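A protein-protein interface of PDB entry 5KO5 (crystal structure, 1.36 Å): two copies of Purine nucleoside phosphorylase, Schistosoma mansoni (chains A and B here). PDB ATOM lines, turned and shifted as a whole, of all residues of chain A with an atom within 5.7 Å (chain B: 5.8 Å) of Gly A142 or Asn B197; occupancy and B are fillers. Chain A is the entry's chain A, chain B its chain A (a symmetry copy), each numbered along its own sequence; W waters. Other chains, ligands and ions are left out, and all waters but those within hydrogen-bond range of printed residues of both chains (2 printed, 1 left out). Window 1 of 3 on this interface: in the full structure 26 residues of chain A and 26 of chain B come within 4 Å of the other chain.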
ATOM      1  N   ASN A 139      23.766   8.774  26.005  1.00  0.00           N
ATOM      2  CA  ASN A 139      24.324  10.127  25.940  1.00  0.00           C
ATOM      3  C   ASN A 139      23.296  11.013  25.252  1.00  0.00           C
ATOM      4  O   ASN A 139      23.357  11.221  24.044  1.00  0.00           O
ATOM      5  CB  ASN A 139      25.606  10.021  25.122  1.00  0.00           C
ATOM      6  CG  ASN A 139      26.347  11.326  24.953  1.00  0.00           C
ATOM      7  OD1 ASN A 139      26.016  12.361  25.538  1.00  0.00           O
ATOM      8  ND2 ASN A 139      27.396  11.277  24.123  1.00  0.00           N
ATOM      9  N   PHE A 140      22.349  11.550  26.026  1.00  0.00           N
ATOM     10  CA  PHE A 140      21.342  12.410  25.414  1.00  0.00           C
ATOM     11  C   PHE A 140      21.952  13.620  24.723  1.00  0.00           C
ATOM     12  O   PHE A 140      21.528  13.923  23.592  1.00  0.00           O
ATOM     13  CB  PHE A 140      20.248  12.768  26.425  1.00  0.00           C
ATOM     14  CG  PHE A 140      19.359  11.601  26.770  1.00  0.00           C
ATOM     15  CD1 PHE A 140      18.356  11.198  25.894  1.00  0.00           C
ATOM     16  CD2 PHE A 140      19.551  10.883  27.939  1.00  0.00           C
ATOM     17  CE1 PHE A 140      17.545  10.114  26.201  1.00  0.00           C
ATOM     18  CE2 PHE A 140      18.748   9.804  28.247  1.00  0.00           C
ATOM     19  CZ  PHE A 140      17.739   9.425  27.380  1.00  0.00           C
ATOM     20  N   PRO A 141      22.929  14.329  25.299  1.00  0.00           N
ATOM     21  CA  PRO A 141      23.577  15.403  24.532  1.00  0.00           C
ATOM     22  C   PRO A 141      24.176  14.908  23.226  1.00  0.00           C
ATOM     23  O   PRO A 141      24.040  15.580  22.193  1.00  0.00           O
ATOM     24  CB  PRO A 141      24.635  15.945  25.515  1.00  0.00           C
ATOM     25  CG  PRO A 141      24.002  15.672  26.890  1.00  0.00           C
ATOM     26  CD  PRO A 141      23.429  14.280  26.693  1.00  0.00           C
ATOM     27  N   GLY A 142      24.825  13.743  23.230  1.00  0.00           N
ATOM     28  CA  GLY A 142      25.418  13.231  22.001  1.00  0.00           C
ATOM     29  C   GLY A 142      24.379  12.958  20.929  1.00  0.00           C
ATOM     30  O   GLY A 142      24.548  13.336  19.766  1.00  0.00           O
ATOM     31  N   LEU A 143      23.292  12.285  21.297  1.00  0.00           N
ATOM     32  CA  LEU A 143      22.234  12.070  20.319  1.00  0.00           C
ATOM     33  C   LEU A 143      21.718  13.398  19.790  1.00  0.00           C
ATOM     34  O   LEU A 143      21.387  13.517  18.601  1.00  0.00           O
ATOM     35  CB  LEU A 143      21.096  11.266  20.947  1.00  0.00           C
ATOM     36  CG  LEU A 143      21.438   9.838  21.390  1.00  0.00           C
ATOM     37  CD1 LEU A 143      20.242   9.243  22.088  1.00  0.00           C
ATOM     38  CD2 LEU A 143      21.819   8.976  20.196  1.00  0.00           C
ATOM     39  N   GLY A 144      21.679  14.418  20.652  1.00  0.00           N
ATOM     40  CA  GLY A 144      21.092  15.710  20.323  1.00  0.00           C
ATOM     41  C   GLY A 144      21.999  16.773  19.730  1.00  0.00           C
ATOM     42  O   GLY A 144      21.652  17.955  19.759  1.00  0.00           O
ATOM     43  N   LEU A 145      23.137  16.383  19.147  1.00  0.00           N
ATOM     44  CA  LEU A 145      24.088  17.281  18.476  1.00  0.00           C
ATOM     45  C   LEU A 145      24.943  18.086  19.443  1.00  0.00           C
ATOM     46  O   LEU A 145      25.608  19.040  19.029  1.00  0.00           O
ATOM     47  CB  LEU A 145      23.488  18.159  17.364  1.00  0.00           C
ATOM     48  CG  LEU A 145      23.684  17.614  15.958  1.00  0.00           C
ATOM     49  CD1 LEU A 145      22.949  18.513  14.964  1.00  0.00           C
ATOM     50  CD2 LEU A 145      25.164  17.515  15.603  1.00  0.00           C
ATOM     51  N   ASN A 146      24.991  17.670  20.712  1.00  0.00           N
ATOM     52  CA  ASN A 146      25.887  18.272  21.694  1.00  0.00           C
ATOM     53  C   ASN A 146      26.941  17.288  22.206  1.00  0.00           C
ATOM     54  O   ASN A 146      27.446  17.438  23.321  1.00  0.00           O
ATOM     55  CB  ASN A 146      25.092  18.902  22.840  1.00  0.00           C
ATOM     56  CG  ASN A 146      24.546  20.272  22.491  1.00  0.00           C
ATOM     57  OD1 ASN A 146      25.109  20.994  21.654  1.00  0.00           O
ATOM     58  ND2 ASN A 146      23.451  20.652  23.133  1.00  0.00           N
ATOM     59  N   ASN A 147      27.302  16.282  21.417  1.00  0.00           N
ATOM     60  CA  ASN A 147      28.401  15.397  21.793  1.00  0.00           C
ATOM     61  C   ASN A 147      29.659  16.232  22.022  1.00  0.00           C
ATOM     62  O   ASN A 147      29.915  17.213  21.310  1.00  0.00           O
ATOM     63  CB  ASN A 147      28.629  14.404  20.646  1.00  0.00           C
ATOM     64  CG  ASN A 147      29.490  13.203  21.027  1.00  0.00           C
ATOM     65  OD1 ASN A 147      30.695  13.333  21.302  1.00  0.00           O
ATOM     66  ND2 ASN A 147      28.882  12.013  20.988  1.00  0.00           N
ATOM     67  N   PHE A 196      23.165  10.342  30.655  1.00  0.00           N
ATOM     68  CA  PHE A 196      23.720  11.686  30.796  1.00  0.00           C
ATOM     69  C   PHE A 196      22.605  12.693  30.535  1.00  0.00           C
ATOM     70  O   PHE A 196      22.124  12.818  29.403  1.00  0.00           O
ATOM     71  CB  PHE A 196      24.882  11.852  29.820  1.00  0.00           C
ATOM     72  CG  PHE A 196      25.549  13.216  29.833  1.00  0.00           C
ATOM     73  CD1 PHE A 196      25.482  14.074  30.935  1.00  0.00           C
ATOM     74  CD2 PHE A 196      26.260  13.634  28.706  1.00  0.00           C
ATOM     75  CE1 PHE A 196      26.107  15.323  30.901  1.00  0.00           C
ATOM     76  CE2 PHE A 196      26.892  14.887  28.673  1.00  0.00           C
ATOM     77  CZ  PHE A 196      26.824  15.729  29.785  1.00  0.00           C
ATOM     78  N   ILE B 138      13.307   9.932  13.611  1.00  0.00           N
ATOM     79  CA  ILE B 138      13.320  10.455  14.975  1.00  0.00           C
ATOM     80  C   ILE B 138      14.533  11.365  15.081  1.00  0.00           C
ATOM     81  O   ILE B 138      15.679  10.907  14.998  1.00  0.00           O
ATOM     82  CB  ILE B 138      13.345   9.354  16.035  1.00  0.00           C
ATOM     83  CG1 ILE B 138      12.076   8.504  15.896  1.00  0.00           C
ATOM     84  CG2 ILE B 138      13.432   9.984  17.432  1.00  0.00           C
ATOM     85  CD1 ILE B 138      11.967   7.369  16.871  1.00  0.00           C
ATOM     86  N   PHE B 140      16.653  13.370  17.111  1.00  0.00           N
ATOM     87  CA  PHE B 140      17.070  13.719  18.465  1.00  0.00           C
ATOM     88  C   PHE B 140      17.615  15.136  18.558  1.00  0.00           C
ATOM     89  O   PHE B 140      17.239  15.845  19.510  1.00  0.00           O
ATOM     90  CB  PHE B 140      18.021  12.659  19.029  1.00  0.00           C
ATOM     91  CG  PHE B 140      17.332  11.355  19.343  1.00  0.00           C
ATOM     92  CD1 PHE B 140      16.569  11.223  20.498  1.00  0.00           C
ATOM     93  CD2 PHE B 140      17.408  10.284  18.468  1.00  0.00           C
ATOM     94  CE1 PHE B 140      15.920  10.030  20.783  1.00  0.00           C
ATOM     95  CE2 PHE B 140      16.763   9.096  18.747  1.00  0.00           C
ATOM     96  CZ  PHE B 140      16.025   8.967  19.909  1.00  0.00           C
ATOM     97  N   PRO B 141      18.456  15.619  17.637  1.00  0.00           N
ATOM     98  CA  PRO B 141      18.843  17.036  17.699  1.00  0.00           C
ATOM     99  C   PRO B 141      17.645  17.970  17.658  1.00  0.00           C
ATOM    100  O   PRO B 141      17.606  18.955  18.411  1.00  0.00           O
ATOM    101  CB  PRO B 141      19.777  17.197  16.482  1.00  0.00           C
ATOM    102  CG  PRO B 141      20.392  15.795  16.330  1.00  0.00           C
ATOM    103  CD  PRO B 141      19.185  14.904  16.563  1.00  0.00           C
ATOM    104  N   TYR B 194      14.425   6.257  10.537  1.00  0.00           N
ATOM    105  CA  TYR B 194      15.821   6.641  10.748  1.00  0.00           C
ATOM    106  C   TYR B 194      15.955   7.492  12.008  1.00  0.00           C
ATOM    107  O   TYR B 194      15.325   8.549  12.125  1.00  0.00           O
ATOM    108  CB  TYR B 194      16.296   7.433   9.529  1.00  0.00           C
ATOM    109  CG  TYR B 194      17.734   7.913   9.516  1.00  0.00           C
ATOM    110  CD1 TYR B 194      18.090   9.113  10.122  1.00  0.00           C
ATOM    111  CD2 TYR B 194      18.712   7.207   8.816  1.00  0.00           C
ATOM    112  CE1 TYR B 194      19.394   9.572  10.074  1.00  0.00           C
ATOM    113  CE2 TYR B 194      20.026   7.659   8.759  1.00  0.00           C
ATOM    114  CZ  TYR B 194      20.354   8.840   9.393  1.00  0.00           C
ATOM    115  OH  TYR B 194      21.640   9.304   9.331  1.00  0.00           O
ATOM    116  N   ALA B 195      16.792   7.053  12.943  1.00  0.00           N
ATOM    117  CA  ALA B 195      17.116   7.880  14.099  1.00  0.00           C
ATOM    118  C   ALA B 195      18.356   8.696  13.781  1.00  0.00           C
ATOM    119  O   ALA B 195      19.373   8.135  13.372  1.00  0.00           O
ATOM    120  CB  ALA B 195      17.411   7.012  15.319  1.00  0.00           C
ATOM    121  N   PHE B 196      18.281  10.013  14.008  1.00  0.00           N
ATOM    122  CA  PHE B 196      19.417  10.907  13.803  1.00  0.00           C
ATOM    123  C   PHE B 196      20.165  11.040  15.126  1.00  0.00           C
ATOM    124  O   PHE B 196      19.648  11.627  16.083  1.00  0.00           O
ATOM    125  CB  PHE B 196      18.909  12.254  13.295  1.00  0.00           C
ATOM    126  CG  PHE B 196      19.980  13.303  13.058  1.00  0.00           C
ATOM    127  CD1 PHE B 196      21.319  12.971  12.827  1.00  0.00           C
ATOM    128  CD2 PHE B 196      19.622  14.653  13.066  1.00  0.00           C
ATOM    129  CE1 PHE B 196      22.273  13.971  12.618  1.00  0.00           C
ATOM    130  CE2 PHE B 196      20.578  15.658  12.852  1.00  0.00           C
ATOM    131  CZ  PHE B 196      21.909  15.309  12.614  1.00  0.00           C
ATOM    132  N   ASN B 197      21.357  10.427  15.184  1.00  0.00           N
ATOM    133  CA  ASN B 197      22.347  10.630  16.242  1.00  0.00           C
ATOM    134  C   ASN B 197      23.315  11.700  15.772  1.00  0.00           C
ATOM    135  O   ASN B 197      24.001  11.518  14.766  1.00  0.00           O
ATOM    136  CB  ASN B 197      23.118   9.324  16.445  1.00  0.00           C
ATOM    137  CG  ASN B 197      24.373   9.496  17.282  1.00  0.00           C
ATOM    138  OD1 ASN B 197      24.441  10.380  18.138  1.00  0.00           O
ATOM    139  ND2 ASN B 197      25.372   8.631  17.054  1.00  0.00           N
ATOM    140  N   GLY B 198      23.361  12.828  16.475  1.00  0.00           N
ATOM    141  CA  GLY B 198      24.262  13.889  16.062  1.00  0.00           C
ATOM    142  C   GLY B 198      25.691  13.421  15.846  1.00  0.00           C
ATOM    143  O   GLY B 198      26.385  13.929  14.970  1.00  0.00           O
ATOM    144  N   GLY B 199      26.163  12.481  16.662  1.00  0.00           N
ATOM    145  CA  GLY B 199      27.513  11.958  16.482  1.00  0.00           C
ATOM    146  C   GLY B 199      28.585  12.882  17.048  1.00  0.00           C
ATOM    147  O   GLY B 199      28.276  13.892  17.675  1.00  0.00           O
ATOM    148  N   PRO B 200      29.861  12.605  16.771  1.00  0.00           N
ATOM    149  CA  PRO B 200      30.370  11.630  15.792  1.00  0.00           C
ATOM    150  C   PRO B 200      30.739  10.282  16.398  1.00  0.00           C
ATOM    151  O   PRO B 200      31.245   9.422  15.670  1.00  0.00           O
ATOM    152  CB  PRO B 200      31.630  12.314  15.269  1.00  0.00           C
ATOM    153  CG  PRO B 200      32.159  13.052  16.511  1.00  0.00           C
ATOM    154  CD  PRO B 200      30.906  13.549  17.222  1.00  0.00           C
ATOM    155  N   THR B 201      30.530  10.076  17.695  1.00  0.00           N
ATOM    156  CA  THR B 201      30.704   8.726  18.225  1.00  0.00           C
ATOM    157  C   THR B 201      29.601   7.838  17.676  1.00  0.00           C
ATOM    158  O   THR B 201      28.438   8.248  17.584  1.00  0.00           O
ATOM    159  CB  THR B 201      30.646   8.692  19.759  1.00  0.00           C
ATOM    160  OG1 THR B 201      29.430   9.290  20.221  1.00  0.00           O
ATOM    161  CG2 THR B 201      31.836   9.424  20.388  1.00  0.00           C
ATOM    162  N   TYR B 202      29.961   6.614  17.291  1.00  0.00           N
ATOM    163  CA  TYR B 202      28.931   5.657  16.924  1.00  0.00           C
ATOM    164  C   TYR B 202      27.970   5.464  18.087  1.00  0.00           C
ATOM    165  O   TYR B 202      28.316   5.678  19.255  1.00  0.00           O
ATOM    166  CB  TYR B 202      29.566   4.317  16.528  1.00  0.00           C
ATOM    167  CG  TYR B 202      30.234   4.364  15.180  1.00  0.00           C
ATOM    168  CD1 TYR B 202      29.483   4.604  14.038  1.00  0.00           C
ATOM    169  CD2 TYR B 202      31.606   4.184  15.040  1.00  0.00           C
ATOM    170  CE1 TYR B 202      30.078   4.654  12.789  1.00  0.00           C
ATOM    171  CE2 TYR B 202      32.214   4.233  13.785  1.00  0.00           C
ATOM    172  CZ  TYR B 202      31.444   4.477  12.673  1.00  0.00           C
ATOM    173  OH  TYR B 202      32.033   4.536  11.425  1.00  0.00           O
ATOM    174  N   GLU B 203      26.753   5.077  17.752  1.00  0.00           N
ATOM    175  CA  GLU B 203      25.776   4.708  18.762  1.00  0.00           C
ATOM    176  C   GLU B 203      26.388   3.712  19.743  1.00  0.00           C
ATOM    177  O   GLU B 203      27.030   2.733  19.342  1.00  0.00           O
ATOM    178  CB  GLU B 203      24.548   4.113  18.056  1.00  0.00           C
ATOM    179  CG  GLU B 203      24.778   2.828  17.212  1.00  0.00           C
ATOM    180  CD  GLU B 203      25.195   3.038  15.748  1.00  0.00           C
ATOM    181  OE1 GLU B 203      25.664   4.130  15.352  1.00  0.00           O
ATOM    182  OE2 GLU B 203      25.066   2.048  14.977  1.00  0.00           O
ATOM    183  N   GLU B 207      22.675   2.872  23.768  1.00  0.00           N
ATOM    184  CA  GLU B 207      21.875   3.724  22.893  1.00  0.00           C
ATOM    185  C   GLU B 207      21.170   2.901  21.826  1.00  0.00           C
ATOM    186  O   GLU B 207      19.981   3.115  21.554  1.00  0.00           O
ATOM    187  CB  GLU B 207      22.754   4.805  22.265  1.00  0.00           C
ATOM    188  CG  GLU B 207      23.207   5.830  23.307  1.00  0.00           C
ATOM    189  CD  GLU B 207      24.437   6.605  22.912  1.00  0.00           C
ATOM    190  OE1 GLU B 207      24.960   6.424  21.795  1.00  0.00           O
ATOM    191  OE2 GLU B 207      24.904   7.399  23.750  1.00  0.00           O
ATOM    192  N   VAL B 219      20.053   3.875  12.455  1.00  0.00           N
ATOM    193  CA  VAL B 219      20.601   5.061  13.117  1.00  0.00           C
ATOM    194  C   VAL B 219      21.790   5.578  12.315  1.00  0.00           C
ATOM    195  O   VAL B 219      22.603   4.797  11.804  1.00  0.00           O
ATOM    196  CB  VAL B 219      20.967   4.781  14.595  1.00  0.00           C
ATOM    197  CG1 VAL B 219      22.025   3.682  14.717  1.00  0.00           C
ATOM    198  CG2 VAL B 219      21.437   6.055  15.299  1.00  0.00           C
ATOM    199  N   GLY B 220      21.889   6.899  12.184  1.00  0.00           N
ATOM    200  CA  GLY B 220      23.045   7.470  11.521  1.00  0.00           C
ATOM    201  C   GLY B 220      23.176   8.929  11.884  1.00  0.00           C
ATOM    202  O   GLY B 220      22.382   9.467  12.658  1.00  0.00           O
ATOM    203  N   MET B 221      24.177   9.573  11.279  1.00  0.00           N
ATOM    204  CA  MET B 221      24.635  10.894  11.705  1.00  0.00           C
ATOM    205  C   MET B 221      24.383  11.981  10.665  1.00  0.00           C
ATOM    206  O   MET B 221      25.029  13.036  10.702  1.00  0.00           O
ATOM    207  CB  MET B 221      26.117  10.864  12.075  1.00  0.00           C
ATOM    208  CG  MET B 221      26.501   9.798  13.071  1.00  0.00           C
ATOM    209  SD  MET B 221      28.288   9.783  13.300  1.00  0.00           S
ATOM    210  CE  MET B 221      28.456   8.252  14.221  1.00  0.00           C
ATOM    211  N   SER B 222      23.459  11.763   9.743  1.00  0.00           N
ATOM    212  CA  SER B 222      23.297  12.719   8.660  1.00  0.00           C
ATOM    213  C   SER B 222      21.837  12.735   8.244  1.00  0.00           C
ATOM    214  O   SER B 222      20.963  12.248   8.969  1.00  0.00           O
ATOM    215  CB  SER B 222      24.202  12.337   7.477  1.00  0.00           C
ATOM    216  OG  SER B 222      23.725  11.156   6.865  1.00  0.00           O
HETATM  217  O   HOH W   1      27.457   8.331  23.280  1.00  0.00           O
HETATM  218  O   HOH W   2      26.435  10.610  20.148  1.00  0.00           O
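OD1 of Asn A139 lies within hydrogen-bond range of N of Gly A142 (2.9 Å). N of Asn A147 is in hydrogen-bond range of O of Pro A141 (3.4 Å). O of Ile B138 sits at hydrogen-bond distance from N of Phe B196 (2.9 Å). The side-chain amide oxygen (OD1) of Asn B197 lies close to the backbone NH (N) of Gly B199 (3.1 Å). ND2 of Asn B197 lies within hydrogen-bond range of O of Thr B201 (3.1 Å). The backbone NH (N) of Asn B197 is in hydrogen-bond range of the backbone carbonyl oxygen (O) of Gly B220, at 2.9 Å.
Positions printed for both chains: 140, 141 and 196.
The backbone NH (N) of Asn A139 sits at hydrogen-bond distance from the side-chain carboxylate (OE2) of Glu B207 (2.9 Å). The backbone carbonyl oxygen (O) of Gly A142 lies close to the side-chain amide oxygen (OD1) of Asn B197, 3.4 Å away. The backbone NH of Gly B198 lies within hydrogen-bond range of the backbone carbonyl oxygen of Leu A143, at 3.0 Å. The side-chain hydroxyl (OG1) of Thr B201 lies within hydrogen-bond range of the side-chain amide nitrogen (ND2) of Asn A147 (2.9 Å).
Among the printed residues, pairs that only touch across the chains: Gly A142 with Gly B198, Gly A142 with Gly B199, Leu A143 with Phe B140, Leu A143 with Pro B141, Leu A143 with Phe B196, Leu A143 with Asn B197, Gly A144 with Phe B140, Gly A144 with Pro B141, Leu A145 with Pro B141, Leu A145 with Gly B198 and Asn A147 with Gly B199.
Water W1 lies within hydrogen-bond range of the side-chain carboxylate (OE2) of Glu B207 (2.8 Å) and the side-chain amide nitrogen (ND2) of Asn A139 (3.1 Å). Water W2 lies within hydrogen-bond range of the side-chain amide oxygen (OD1) of Asn B197 (2.8 Å), the side-chain amide nitrogen (ND2) of Asn A147 (2.9 Å), the side-chain hydroxyl (OG1) of Thr B201 (3.3 Å) and the backbone carbonyl oxygen (O) of Gly A142 (3.3 Å).
Pro A141 touches none of the printed residues of chain B. Of chain B, only Asn B197 (3.4 Å), Gly B198 (3.5 Å) and Gly B199 (3.6 Å) come within 4 Å of Gly A142. Of the printed residues of chain B, Leu A143 touches Phe B140 (3.5 Å), Pro B141 (3.3 Å), Phe B196 (3.6 Å), Asn B197 (3.5 Å) and Gly B198 (3.0 Å). Of the printed residues of chain A, Gly B198 touches Gly A142, Leu A143 and Leu A145. Of the printed residues of chain A, Gly B199 touches Gly A142 (3.6 Å) and Asn A147 (3.0 Å). Gly B220 touches none of the printed residues of chain A. The nearest printed residue of chain A that does not touch Asn B197 is Gly A144 (5.5 Å).
Of the 10 printed residues of chain A, 6 touch a printed residue of chain B. Printed residues of chain A that touch a printed residue of chain B: Asn A139, Gly A142, Leu A143, Gly A144, Leu A145 and Asn A147. Among the printed residues, no Asp or Glu carboxylate lies within 4 Å of a Lys or Arg side-chain nitrogen of the other chain.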
